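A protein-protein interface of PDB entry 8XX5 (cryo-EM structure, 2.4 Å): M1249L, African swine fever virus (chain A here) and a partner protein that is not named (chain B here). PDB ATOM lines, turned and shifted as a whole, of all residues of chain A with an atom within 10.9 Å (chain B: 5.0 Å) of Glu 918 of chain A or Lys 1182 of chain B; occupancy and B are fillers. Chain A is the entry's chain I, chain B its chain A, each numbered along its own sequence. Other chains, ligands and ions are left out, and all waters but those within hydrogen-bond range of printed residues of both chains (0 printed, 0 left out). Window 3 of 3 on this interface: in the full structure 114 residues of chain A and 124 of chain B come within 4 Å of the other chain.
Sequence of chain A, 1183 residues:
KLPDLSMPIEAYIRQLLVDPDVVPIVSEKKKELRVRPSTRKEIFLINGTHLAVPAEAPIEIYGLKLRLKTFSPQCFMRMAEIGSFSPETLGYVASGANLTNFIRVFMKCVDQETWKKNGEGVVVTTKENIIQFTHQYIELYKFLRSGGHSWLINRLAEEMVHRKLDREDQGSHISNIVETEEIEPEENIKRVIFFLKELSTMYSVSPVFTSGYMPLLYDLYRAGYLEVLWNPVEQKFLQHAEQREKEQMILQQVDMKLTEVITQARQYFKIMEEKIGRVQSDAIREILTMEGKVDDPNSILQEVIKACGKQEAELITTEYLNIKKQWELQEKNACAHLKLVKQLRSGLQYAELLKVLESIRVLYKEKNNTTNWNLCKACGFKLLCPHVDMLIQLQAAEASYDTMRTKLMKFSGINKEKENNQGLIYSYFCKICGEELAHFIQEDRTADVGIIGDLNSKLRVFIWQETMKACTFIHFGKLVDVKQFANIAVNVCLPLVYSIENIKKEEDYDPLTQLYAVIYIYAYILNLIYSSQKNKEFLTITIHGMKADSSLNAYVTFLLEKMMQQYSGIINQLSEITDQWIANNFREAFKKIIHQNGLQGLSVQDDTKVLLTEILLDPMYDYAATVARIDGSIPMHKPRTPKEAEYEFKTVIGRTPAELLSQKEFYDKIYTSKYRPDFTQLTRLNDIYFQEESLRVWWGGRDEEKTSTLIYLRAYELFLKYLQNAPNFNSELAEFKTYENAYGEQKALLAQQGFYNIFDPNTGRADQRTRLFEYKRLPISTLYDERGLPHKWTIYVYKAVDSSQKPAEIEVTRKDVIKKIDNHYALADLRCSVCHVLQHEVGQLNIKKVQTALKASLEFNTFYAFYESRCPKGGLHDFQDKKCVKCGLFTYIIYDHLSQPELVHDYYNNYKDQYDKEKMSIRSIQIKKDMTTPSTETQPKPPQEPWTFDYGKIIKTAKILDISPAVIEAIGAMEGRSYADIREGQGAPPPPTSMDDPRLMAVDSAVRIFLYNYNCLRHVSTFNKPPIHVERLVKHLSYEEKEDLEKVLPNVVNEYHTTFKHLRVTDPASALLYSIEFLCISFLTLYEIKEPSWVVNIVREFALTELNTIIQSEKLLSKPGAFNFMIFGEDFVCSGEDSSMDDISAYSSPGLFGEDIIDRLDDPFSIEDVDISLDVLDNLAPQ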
ATOM      1  N   PHE A 866       0.122   4.698 -24.557  1.00  0.00           N
ATOM      2  CA  PHE A 866      -0.252   3.355 -24.979  1.00  0.00           C
ATOM      3  C   PHE A 866      -1.581   3.369 -25.723  1.00  0.00           C
ATOM      4  O   PHE A 866      -1.740   2.678 -26.734  1.00  0.00           O
ATOM      5  CB  PHE A 866      -0.319   2.423 -23.770  1.00  0.00           C
ATOM      6  CG  PHE A 866      -0.482   0.976 -24.131  1.00  0.00           C
ATOM      7  CD1 PHE A 866       0.614   0.212 -24.490  1.00  0.00           C
ATOM      8  CD2 PHE A 866      -1.731   0.381 -24.115  1.00  0.00           C
ATOM      9  CE1 PHE A 866       0.467  -1.120 -24.826  1.00  0.00           C
ATOM     10  CE2 PHE A 866      -1.884  -0.950 -24.449  1.00  0.00           C
ATOM     11  CZ  PHE A 866      -0.784  -1.701 -24.805  1.00  0.00           C
ATOM     12  N   TYR A 867      -2.542   4.160 -25.248  1.00  0.00           N
ATOM     13  CA  TYR A 867      -3.880   4.196 -25.818  1.00  0.00           C
ATOM     14  C   TYR A 867      -4.141   5.450 -26.646  1.00  0.00           C
ATOM     15  O   TYR A 867      -5.303   5.806 -26.863  1.00  0.00           O
ATOM     16  CB  TYR A 867      -4.928   4.070 -24.712  1.00  0.00           C
ATOM     17  CG  TYR A 867      -5.032   2.684 -24.125  1.00  0.00           C
ATOM     18  CD1 TYR A 867      -5.071   1.563 -24.944  1.00  0.00           C
ATOM     19  CD2 TYR A 867      -5.099   2.493 -22.753  1.00  0.00           C
ATOM     20  CE1 TYR A 867      -5.172   0.294 -24.414  1.00  0.00           C
ATOM     21  CE2 TYR A 867      -5.199   1.228 -22.213  1.00  0.00           C
ATOM     22  CZ  TYR A 867      -5.235   0.131 -23.047  1.00  0.00           C
ATOM     23  OH  TYR A 867      -5.334  -1.132 -22.512  1.00  0.00           O
ATOM     24  N   ARG A 870      -4.020   2.876 -29.807  1.00  0.00           N
ATOM     25  CA  ARG A 870      -4.560   1.584 -29.412  1.00  0.00           C
ATOM     26  C   ARG A 870      -5.881   1.772 -28.681  1.00  0.00           C
ATOM     27  O   ARG A 870      -6.023   2.658 -27.836  1.00  0.00           O
ATOM     28  CB  ARG A 870      -3.574   0.845 -28.507  1.00  0.00           C
ATOM     29  CG  ARG A 870      -2.310   0.362 -29.191  1.00  0.00           C
ATOM     30  CD  ARG A 870      -1.306  -0.140 -28.168  1.00  0.00           C
ATOM     31  NE  ARG A 870      -0.012  -0.440 -28.765  1.00  0.00           N
ATOM     32  CZ  ARG A 870       1.114   0.195 -28.468  1.00  0.00           C
ATOM     33  NH1 ARG A 870       1.137   1.189 -27.597  1.00  0.00           N
ATOM     34  NH2 ARG A 870       2.244  -0.178 -29.061  1.00  0.00           N
ATOM     35  N   CYS A 871      -6.845   0.934 -29.007  1.00  0.00           N
ATOM     36  CA  CYS A 871      -8.099   1.018 -28.277  1.00  0.00           C
ATOM     37  C   CYS A 871      -8.126  -0.024 -27.175  1.00  0.00           C
ATOM     38  O   CYS A 871      -7.800  -1.193 -27.432  1.00  0.00           O
ATOM     39  CB  CYS A 871      -9.285   0.811 -29.212  1.00  0.00           C
ATOM     40  SG  CYS A 871     -10.874   1.305 -28.512  1.00  0.00           S
ATOM     41  N   PRO A 872      -8.473   0.353 -25.943  1.00  0.00           N
ATOM     42  CA  PRO A 872      -8.696  -0.668 -24.910  1.00  0.00           C
ATOM     43  C   PRO A 872      -9.788  -1.651 -25.286  1.00  0.00           C
ATOM     44  O   PRO A 872      -9.712  -2.826 -24.906  1.00  0.00           O
ATOM     45  CB  PRO A 872      -9.073   0.161 -23.676  1.00  0.00           C
ATOM     46  CG  PRO A 872      -8.493   1.509 -23.930  1.00  0.00           C
ATOM     47  CD  PRO A 872      -8.582   1.720 -25.410  1.00  0.00           C
ATOM     48  N   LYS A 873     -10.810  -1.199 -26.018  1.00  0.00           N
ATOM     49  CA  LYS A 873     -11.756  -2.131 -26.619  1.00  0.00           C
ATOM     50  C   LYS A 873     -11.059  -3.030 -27.633  1.00  0.00           C
ATOM     51  O   LYS A 873     -11.312  -4.240 -27.680  1.00  0.00           O
ATOM     52  CB  LYS A 873     -12.901  -1.365 -27.280  1.00  0.00           C
ATOM     53  CG  LYS A 873     -14.239  -2.088 -27.263  1.00  0.00           C
ATOM     54  CD  LYS A 873     -14.706  -2.360 -25.842  1.00  0.00           C
ATOM     55  CE  LYS A 873     -14.973  -1.065 -25.096  1.00  0.00           C
ATOM     56  NZ  LYS A 873     -15.178  -1.296 -23.640  1.00  0.00           N
ATOM     57  N   GLY A 874     -10.178  -2.456 -28.449  1.00  0.00           N
ATOM     58  CA  GLY A 874      -9.375  -3.234 -29.372  1.00  0.00           C
ATOM     59  C   GLY A 874      -9.487  -2.816 -30.823  1.00  0.00           C
ATOM     60  O   GLY A 874     -10.586  -2.785 -31.385  1.00  0.00           O
ATOM     61  N   GLY A 875      -8.354  -2.488 -31.441  1.00  0.00           N
ATOM     62  CA  GLY A 875      -8.306  -2.263 -32.873  1.00  0.00           C
ATOM     63  C   GLY A 875      -8.423  -0.827 -33.342  1.00  0.00           C
ATOM     64  O   GLY A 875      -9.221  -0.533 -34.237  1.00  0.00           O
ATOM     65  N   ASN A 910      -7.174  -1.683 -14.989  1.00  0.00           N
ATOM     66  CA  ASN A 910      -6.767  -3.078 -14.869  1.00  0.00           C
ATOM     67  C   ASN A 910      -6.475  -3.708 -16.226  1.00  0.00           C
ATOM     68  O   ASN A 910      -5.619  -4.596 -16.314  1.00  0.00           O
ATOM     69  CB  ASN A 910      -7.823  -3.881 -14.103  1.00  0.00           C
ATOM     70  CG  ASN A 910      -9.029  -4.225 -14.947  1.00  0.00           C
ATOM     71  OD1 ASN A 910      -9.466  -3.434 -15.775  1.00  0.00           O
ATOM     72  ND2 ASN A 910      -9.574  -5.418 -14.742  1.00  0.00           N
ATOM     73  N   TYR A 911      -7.153  -3.266 -17.291  1.00  0.00           N
ATOM     74  CA  TYR A 911      -6.786  -3.727 -18.627  1.00  0.00           C
ATOM     75  C   TYR A 911      -5.354  -3.327 -18.960  1.00  0.00           C
ATOM     76  O   TYR A 911      -4.563  -4.144 -19.443  1.00  0.00           O
ATOM     77  CB  TYR A 911      -7.741  -3.181 -19.696  1.00  0.00           C
ATOM     78  CG  TYR A 911      -9.212  -3.102 -19.335  1.00  0.00           C
ATOM     79  CD1 TYR A 911      -9.684  -2.165 -18.428  1.00  0.00           C
ATOM     80  CD2 TYR A 911     -10.134  -3.957 -19.928  1.00  0.00           C
ATOM     81  CE1 TYR A 911     -11.028  -2.091 -18.106  1.00  0.00           C
ATOM     82  CE2 TYR A 911     -11.478  -3.889 -19.615  1.00  0.00           C
ATOM     83  CZ  TYR A 911     -11.919  -2.954 -18.704  1.00  0.00           C
ATOM     84  OH  TYR A 911     -13.256  -2.881 -18.388  1.00  0.00           O
ATOM     85  N   LYS A 912      -4.999  -2.067 -18.697  1.00  0.00           N
ATOM     86  CA  LYS A 912      -3.633  -1.625 -18.951  1.00  0.00           C
ATOM     87  C   LYS A 912      -2.642  -2.404 -18.096  1.00  0.00           C
ATOM     88  O   LYS A 912      -1.560  -2.774 -18.566  1.00  0.00           O
ATOM     89  CB  LYS A 912      -3.509  -0.122 -18.694  1.00  0.00           C
ATOM     90  CG  LYS A 912      -2.075   0.380 -18.622  1.00  0.00           C
ATOM     91  CD  LYS A 912      -1.527   0.685 -20.006  1.00  0.00           C
ATOM     92  CE  LYS A 912      -0.197   1.414 -19.924  1.00  0.00           C
ATOM     93  NZ  LYS A 912      -0.037   2.142 -18.635  1.00  0.00           N
ATOM     94  N   ASP A 913      -3.004  -2.678 -16.841  1.00  0.00           N
ATOM     95  CA  ASP A 913      -2.114  -3.421 -15.955  1.00  0.00           C
ATOM     96  C   ASP A 913      -1.863  -4.832 -16.474  1.00  0.00           C
ATOM     97  O   ASP A 913      -0.717  -5.297 -16.515  1.00  0.00           O
ATOM     98  CB  ASP A 913      -2.702  -3.461 -14.544  1.00  0.00           C
ATOM     99  CG  ASP A 913      -2.363  -2.226 -13.736  1.00  0.00           C
ATOM    100  OD1 ASP A 913      -2.067  -1.177 -14.346  1.00  0.00           O
ATOM    101  OD2 ASP A 913      -2.392  -2.301 -12.489  1.00  0.00           O
ATOM    102  N   GLN A 914      -2.924  -5.533 -16.885  1.00  0.00           N
ATOM    103  CA  GLN A 914      -2.743  -6.903 -17.356  1.00  0.00           C
ATOM    104  C   GLN A 914      -2.014  -6.937 -18.695  1.00  0.00           C
ATOM    105  O   GLN A 914      -1.220  -7.849 -18.948  1.00  0.00           O
ATOM    106  CB  GLN A 914      -4.086  -7.632 -17.453  1.00  0.00           C
ATOM    107  CG  GLN A 914      -5.122  -6.971 -18.336  1.00  0.00           C
ATOM    108  CD  GLN A 914      -6.152  -7.955 -18.850  1.00  0.00           C
ATOM    109  OE1 GLN A 914      -5.885  -9.151 -18.951  1.00  0.00           O
ATOM    110  NE2 GLN A 914      -7.339  -7.455 -19.175  1.00  0.00           N
ATOM    111  N   TYR A 915      -2.264  -5.955 -19.566  1.00  0.00           N
ATOM    112  CA  TYR A 915      -1.510  -5.878 -20.814  1.00  0.00           C
ATOM    113  C   TYR A 915      -0.030  -5.630 -20.551  1.00  0.00           C
ATOM    114  O   TYR A 915       0.832  -6.212 -21.220  1.00  0.00           O
ATOM    115  CB  TYR A 915      -2.091  -4.796 -21.730  1.00  0.00           C
ATOM    116  CG  TYR A 915      -3.442  -5.124 -22.348  1.00  0.00           C
ATOM    117  CD1 TYR A 915      -4.347  -5.967 -21.716  1.00  0.00           C
ATOM    118  CD2 TYR A 915      -3.785  -4.625 -23.599  1.00  0.00           C
ATOM    119  CE1 TYR A 915      -5.567  -6.267 -22.286  1.00  0.00           C
ATOM    120  CE2 TYR A 915      -5.004  -4.921 -24.179  1.00  0.00           C
ATOM    121  CZ  TYR A 915      -5.890  -5.745 -23.518  1.00  0.00           C
ATOM    122  OH  TYR A 915      -7.104  -6.050 -24.089  1.00  0.00           O
ATOM    123  N   ASP A 916       0.288  -4.768 -19.581  1.00  0.00           N
ATOM    124  CA  ASP A 916       1.684  -4.564 -19.207  1.00  0.00           C
ATOM    125  C   ASP A 916       2.298  -5.845 -18.660  1.00  0.00           C
ATOM    126  O   ASP A 916       3.456  -6.164 -18.956  1.00  0.00           O
ATOM    127  CB  ASP A 916       1.799  -3.437 -18.180  1.00  0.00           C
ATOM    128  CG  ASP A 916       1.620  -2.066 -18.799  1.00  0.00           C
ATOM    129  OD1 ASP A 916       1.014  -1.978 -19.887  1.00  0.00           O
ATOM    130  OD2 ASP A 916       2.088  -1.077 -18.197  1.00  0.00           O
ATOM    131  N   LYS A 917       1.539  -6.588 -17.851  1.00  0.00           N
ATOM    132  CA  LYS A 917       2.042  -7.853 -17.323  1.00  0.00           C
ATOM    133  C   LYS A 917       2.328  -8.846 -18.443  1.00  0.00           C
ATOM    134  O   LYS A 917       3.365  -9.519 -18.436  1.00  0.00           O
ATOM    135  CB  LYS A 917       1.040  -8.442 -16.330  1.00  0.00           C
ATOM    136  CG  LYS A 917       0.968  -7.706 -15.005  1.00  0.00           C
ATOM    137  CD  LYS A 917       1.199  -8.650 -13.835  1.00  0.00           C
ATOM    138  CE  LYS A 917       1.994  -7.973 -12.729  1.00  0.00           C
ATOM    139  NZ  LYS A 917       2.493  -8.948 -11.720  1.00  0.00           N
ATOM    140  N   GLU A 918       1.419  -8.950 -19.416  1.00  0.00           N
ATOM    141  CA  GLU A 918       1.616  -9.887 -20.519  1.00  0.00           C
ATOM    142  C   GLU A 918       2.785  -9.474 -21.405  1.00  0.00           C
ATOM    143  O   GLU A 918       3.555 -10.326 -21.862  1.00  0.00           O
ATOM    144  CB  GLU A 918       0.336 -10.005 -21.348  1.00  0.00           C
ATOM    145  CG  GLU A 918      -0.879 -10.474 -20.563  1.00  0.00           C
ATOM    146  CD  GLU A 918      -2.047 -10.836 -21.458  1.00  0.00           C
ATOM    147  OE1 GLU A 918      -1.809 -11.406 -22.543  1.00  0.00           O
ATOM    148  OE2 GLU A 918      -3.202 -10.548 -21.081  1.00  0.00           O
ATOM    149  N   LYS A 919       2.930  -8.172 -21.664  1.00  0.00           N
ATOM    150  CA  LYS A 919       3.972  -7.708 -22.574  1.00  0.00           C
ATOM    151  C   LYS A 919       5.365  -7.986 -22.021  1.00  0.00           C
ATOM    152  O   LYS A 919       6.250  -8.454 -22.748  1.00  0.00           O
ATOM    153  CB  LYS A 919       3.793  -6.216 -22.854  1.00  0.00           C
ATOM    154  CG  LYS A 919       4.801  -5.651 -23.833  1.00  0.00           C
ATOM    155  CD  LYS A 919       5.591  -4.516 -23.206  1.00  0.00           C
ATOM    156  CE  LYS A 919       7.018  -4.481 -23.724  1.00  0.00           C
ATOM    157  NZ  LYS A 919       7.698  -3.202 -23.386  1.00  0.00           N
ATOM    158  N   MET A 920       5.581  -7.704 -20.738  1.00  0.00           N
ATOM    159  CA  MET A 920       6.903  -7.847 -20.126  1.00  0.00           C
ATOM    160  C   MET A 920       7.069  -9.240 -19.518  1.00  0.00           C
ATOM    161  O   MET A 920       7.231  -9.416 -18.310  1.00  0.00           O
ATOM    162  CB  MET A 920       7.121  -6.755 -19.084  1.00  0.00           C
ATOM    163  CG  MET A 920       7.817  -5.513 -19.620  1.00  0.00           C
ATOM    164  SD  MET A 920       9.132  -5.898 -20.792  1.00  0.00           S
ATOM    165  CE  MET A 920       9.862  -4.281 -21.030  1.00  0.00           C
ATOM    166  N   SER A 921       7.030 -10.243 -20.389  1.00  0.00           N
ATOM    167  CA  SER A 921       7.161 -11.632 -19.966  1.00  0.00           C
ATOM    168  C   SER A 921       7.609 -12.518 -21.121  1.00  0.00           C
ATOM    169  O   SER A 921       7.331 -12.225 -22.284  1.00  0.00           O
ATOM    170  CB  SER A 921       5.838 -12.144 -19.390  1.00  0.00           C
ATOM    171  OG  SER A 921       4.969 -12.583 -20.418  1.00  0.00           O
ATOM    172  N   LEU B1180      -1.003 -17.765 -31.962  1.00  0.00           N
ATOM    173  CA  LEU B1180      -0.917 -16.316 -32.066  1.00  0.00           C
ATOM    174  C   LEU B1180       0.018 -15.764 -30.999  1.00  0.00           C
ATOM    175  O   LEU B1180       0.000 -16.206 -29.847  1.00  0.00           O
ATOM    176  CB  LEU B1180      -2.303 -15.684 -31.922  1.00  0.00           C
ATOM    177  CG  LEU B1180      -3.380 -16.065 -32.942  1.00  0.00           C
ATOM    178  CD1 LEU B1180      -4.424 -14.966 -33.051  1.00  0.00           C
ATOM    179  CD2 LEU B1180      -2.773 -16.357 -34.303  1.00  0.00           C
ATOM    180  N   ASN B1181       0.840 -14.792 -31.389  1.00  0.00           N
ATOM    181  CA  ASN B1181       1.724 -14.108 -30.453  1.00  0.00           C
ATOM    182  C   ASN B1181       0.924 -13.023 -29.741  1.00  0.00           C
ATOM    183  O   ASN B1181       0.493 -12.050 -30.366  1.00  0.00           O
ATOM    184  CB  ASN B1181       2.929 -13.522 -31.183  1.00  0.00           C
ATOM    185  CG  ASN B1181       3.976 -12.965 -30.234  1.00  0.00           C
ATOM    186  OD1 ASN B1181       3.997 -13.302 -29.052  1.00  0.00           O
ATOM    187  ND2 ASN B1181       4.847 -12.106 -30.749  1.00  0.00           N
ATOM    188  N   LYS B1182       0.718 -13.194 -28.433  1.00  0.00           N
ATOM    189  CA  LYS B1182      -0.111 -12.251 -27.691  1.00  0.00           C
ATOM    190  C   LYS B1182       0.615 -10.928 -27.469  1.00  0.00           C
ATOM    191  O   LYS B1182      -0.020  -9.869 -27.458  1.00  0.00           O
ATOM    192  CB  LYS B1182      -0.532 -12.871 -26.356  1.00  0.00           C
ATOM    193  CG  LYS B1182      -1.694 -12.183 -25.629  1.00  0.00           C
ATOM    194  CD  LYS B1182      -2.545 -11.308 -26.543  1.00  0.00           C
ATOM    195  CE  LYS B1182      -3.825 -10.863 -25.855  1.00  0.00           C
ATOM    196  NZ  LYS B1182      -4.645  -9.985 -26.736  1.00  0.00           N
ATOM    197  N   THR B1183       1.938 -10.964 -27.293  1.00  0.00           N
ATOM    198  CA  THR B1183       2.691  -9.725 -27.119  1.00  0.00           C
ATOM    199  C   THR B1183       2.570  -8.831 -28.348  1.00  0.00           C
ATOM    200  O   THR B1183       2.321  -7.624 -28.228  1.00  0.00           O
ATOM    201  CB  THR B1183       4.160 -10.037 -26.829  1.00  0.00           C
ATOM    202  OG1 THR B1183       4.269 -10.703 -25.564  1.00  0.00           O
ATOM    203  CG2 THR B1183       4.988  -8.762 -26.801  1.00  0.00           C
ATOM    204  N   THR B1184       2.723  -9.412 -29.539  1.00  0.00           N
ATOM    205  CA  THR B1184       2.597  -8.632 -30.765  1.00  0.00           C
ATOM    206  C   THR B1184       1.164  -8.146 -30.959  1.00  0.00           C
ATOM    207  O   THR B1184       0.937  -7.010 -31.393  1.00  0.00           O
ATOM    208  CB  THR B1184       3.060  -9.468 -31.960  1.00  0.00           C
ATOM    209  OG1 THR B1184       4.489  -9.562 -31.947  1.00  0.00           O
ATOM    210  CG2 THR B1184       2.639  -8.820 -33.258  1.00  0.00           C
ATOM    211  N   MET B1185       0.183  -8.987 -30.621  1.00  0.00           N
ATOM    212  CA  MET B1185      -1.216  -8.583 -30.728  1.00  0.00           C
ATOM    213  C   MET B1185      -1.516  -7.392 -29.826  1.00  0.00           C
ATOM    214  O   MET B1185      -2.241  -6.471 -30.219  1.00  0.00           O
ATOM    215  CB  MET B1185      -2.127  -9.759 -30.375  1.00  0.00           C
ATOM    216  CG  MET B1185      -2.936 -10.303 -31.538  1.00  0.00           C
ATOM    217  SD  MET B1185      -3.596 -11.947 -31.209  1.00  0.00           S
ATOM    218  CE  MET B1185      -5.002 -11.546 -30.175  1.00  0.00           C
ATOM    219  N   ILE B1186      -0.974  -7.401 -28.608  1.00  0.00           N
ATOM    220  CA  ILE B1186      -1.175  -6.285 -27.690  1.00  0.00           C
ATOM    221  C   ILE B1186      -0.476  -5.033 -28.209  1.00  0.00           C
ATOM    222  O   ILE B1186      -1.061  -3.945 -28.246  1.00  0.00           O
ATOM    223  CB  ILE B1186      -0.685  -6.659 -26.279  1.00  0.00           C
ATOM    224  CG1 ILE B1186      -1.672  -7.615 -25.606  1.00  0.00           C
ATOM    225  CG2 ILE B1186      -0.469  -5.413 -25.432  1.00  0.00           C
ATOM    226  CD1 ILE B1186      -1.031  -8.534 -24.593  1.00  0.00           C
ATOM    227  N   LEU B1187       0.787  -5.171 -28.624  1.00  0.00           N
ATOM    228  CA  LEU B1187       1.554  -4.002 -29.043  1.00  0.00           C
ATOM    229  C   LEU B1187       1.007  -3.386 -30.324  1.00  0.00           C
ATOM    230  O   LEU B1187       1.031  -2.159 -30.476  1.00  0.00           O
ATOM    231  CB  LEU B1187       3.026  -4.373 -29.219  1.00  0.00           C
ATOM    232  CG  LEU B1187       3.788  -4.711 -27.935  1.00  0.00           C
ATOM    233  CD1 LEU B1187       5.173  -5.245 -28.260  1.00  0.00           C
ATOM    234  CD2 LEU B1187       3.880  -3.493 -27.027  1.00  0.00           C
ATOM    235  N   THR B1215      -8.196 -15.709 -23.387  1.00  0.00           N
ATOM    236  CA  THR B1215      -6.894 -16.205 -22.945  1.00  0.00           C
ATOM    237  C   THR B1215      -6.050 -15.159 -22.227  1.00  0.00           C
ATOM    238  O   THR B1215      -5.762 -14.093 -22.779  1.00  0.00           O
ATOM    239  CB  THR B1215      -6.089 -16.738 -24.134  1.00  0.00           C
ATOM    240  OG1 THR B1215      -5.542 -15.640 -24.875  1.00  0.00           O
ATOM    241  CG2 THR B1215      -6.947 -17.600 -25.040  1.00  0.00           C
ATOM    242  N   ALA B1216      -5.643 -15.468 -21.000  1.00  0.00           N
ATOM    243  CA  ALA B1216      -4.701 -14.644 -20.261  1.00  0.00           C
ATOM    244  C   ALA B1216      -3.284 -15.145 -20.535  1.00  0.00           C
ATOM    245  O   ALA B1216      -3.051 -15.953 -21.438  1.00  0.00           O
ATOM    246  CB  ALA B1216      -5.041 -14.655 -18.772  1.00  0.00           C
ATOM    247  N   SER B1217      -2.315 -14.663 -19.761  1.00  0.00           N
ATOM    248  CA  SER B1217      -0.928 -15.103 -19.905  1.00  0.00           C
ATOM    249  C   SER B1217      -0.805 -16.524 -19.370  1.00  0.00           C
ATOM    250  O   SER B1217      -0.979 -16.771 -18.175  1.00  0.00           O
ATOM    251  CB  SER B1217       0.013 -14.154 -19.172  1.00  0.00           C
ATOM    252  OG  SER B1217       1.267 -14.769 -18.930  1.00  0.00           O
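O of Leu 1187 of chain B is in hydrogen-bond range of NE of Arg 870 of chain A (2.6 Å).
The backbone carbonyl oxygen (O) of Phe 866 of chain A lies close to the guanidinium group (NH1) of Arg 870 of chain A, at 3.4 Å.
O of Glu 918 of chain A lies within hydrogen-bond range of OG of Ser 921 of chain A, 3.0 Å away.
Phe 866 of chain A touches Ile 1186 of chain B (CZ to CG2, 3.8 Å).
Arg 870 of chain A touches Ile 1186 of chain B.
CD2 of Tyr 915 of chain A touches CG2 of Ile 1186 of chain B (3.9 Å).
CG of Lys 1182 of chain B touches OE1 of Glu 918 of chain A (3.2 Å).
Thr 1183 of chain B touches Glu 918 of chain A (OG1 to O, 3.8 Å).
Ile 1186 of chain B touches Glu 918 of chain A (CD1 to OE1, 3.6 Å).
CG of Lys 919 of chain A touches CD2 of Leu 1187 of chain B, at 3.96 Å.
Glu 918 of chain A touches three residues of chain B.
Of chain A, only Glu 918 (3.2 Å) comes within 4 Å of Lys 1182 of chain B.
No residue of chain A comes within 4 Å of Met 1185 of chain B.
Ile 1186 of chain B touches just these residues of chain A: Phe 866 (3.8 Å), Arg 870 (3.7 Å), Tyr 915 (3.9 Å) and Glu 918 (3.6 Å).
No residue of chain A comes within 4 Å of Ser 1217 of chain B.
Printed residues of chain B within 4 Å of Arg 870 of chain A: Ile 1186 (3.7 Å) and Leu 1187 (2.6 Å).
Printed residues of chain B within 4 Å of Tyr 915 of chain A: Ile 1186 (3.9 Å).
Of the printed residues of chain A, Leu 1187 of chain B touches Arg 870 (2.6 Å) and Lys 919 (3.96 Å).
Of the printed residues of chain B, Lys 919 of chain A touches Leu 1187 (3.96 Å).
The nearest residue of chain B that does not touch Glu 918 of chain A is Ser 1217 of chain B (4.03 Å).
Hydrophobic or aromatic side chains of chain B within 4 Å of the printed part of chain A: Ile 1186 and Leu 1187.
Of the 20 printed residues of chain A, 5 touch a printed residue of chain B.
Among the printed residues, 8 pairs touch across the chains.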
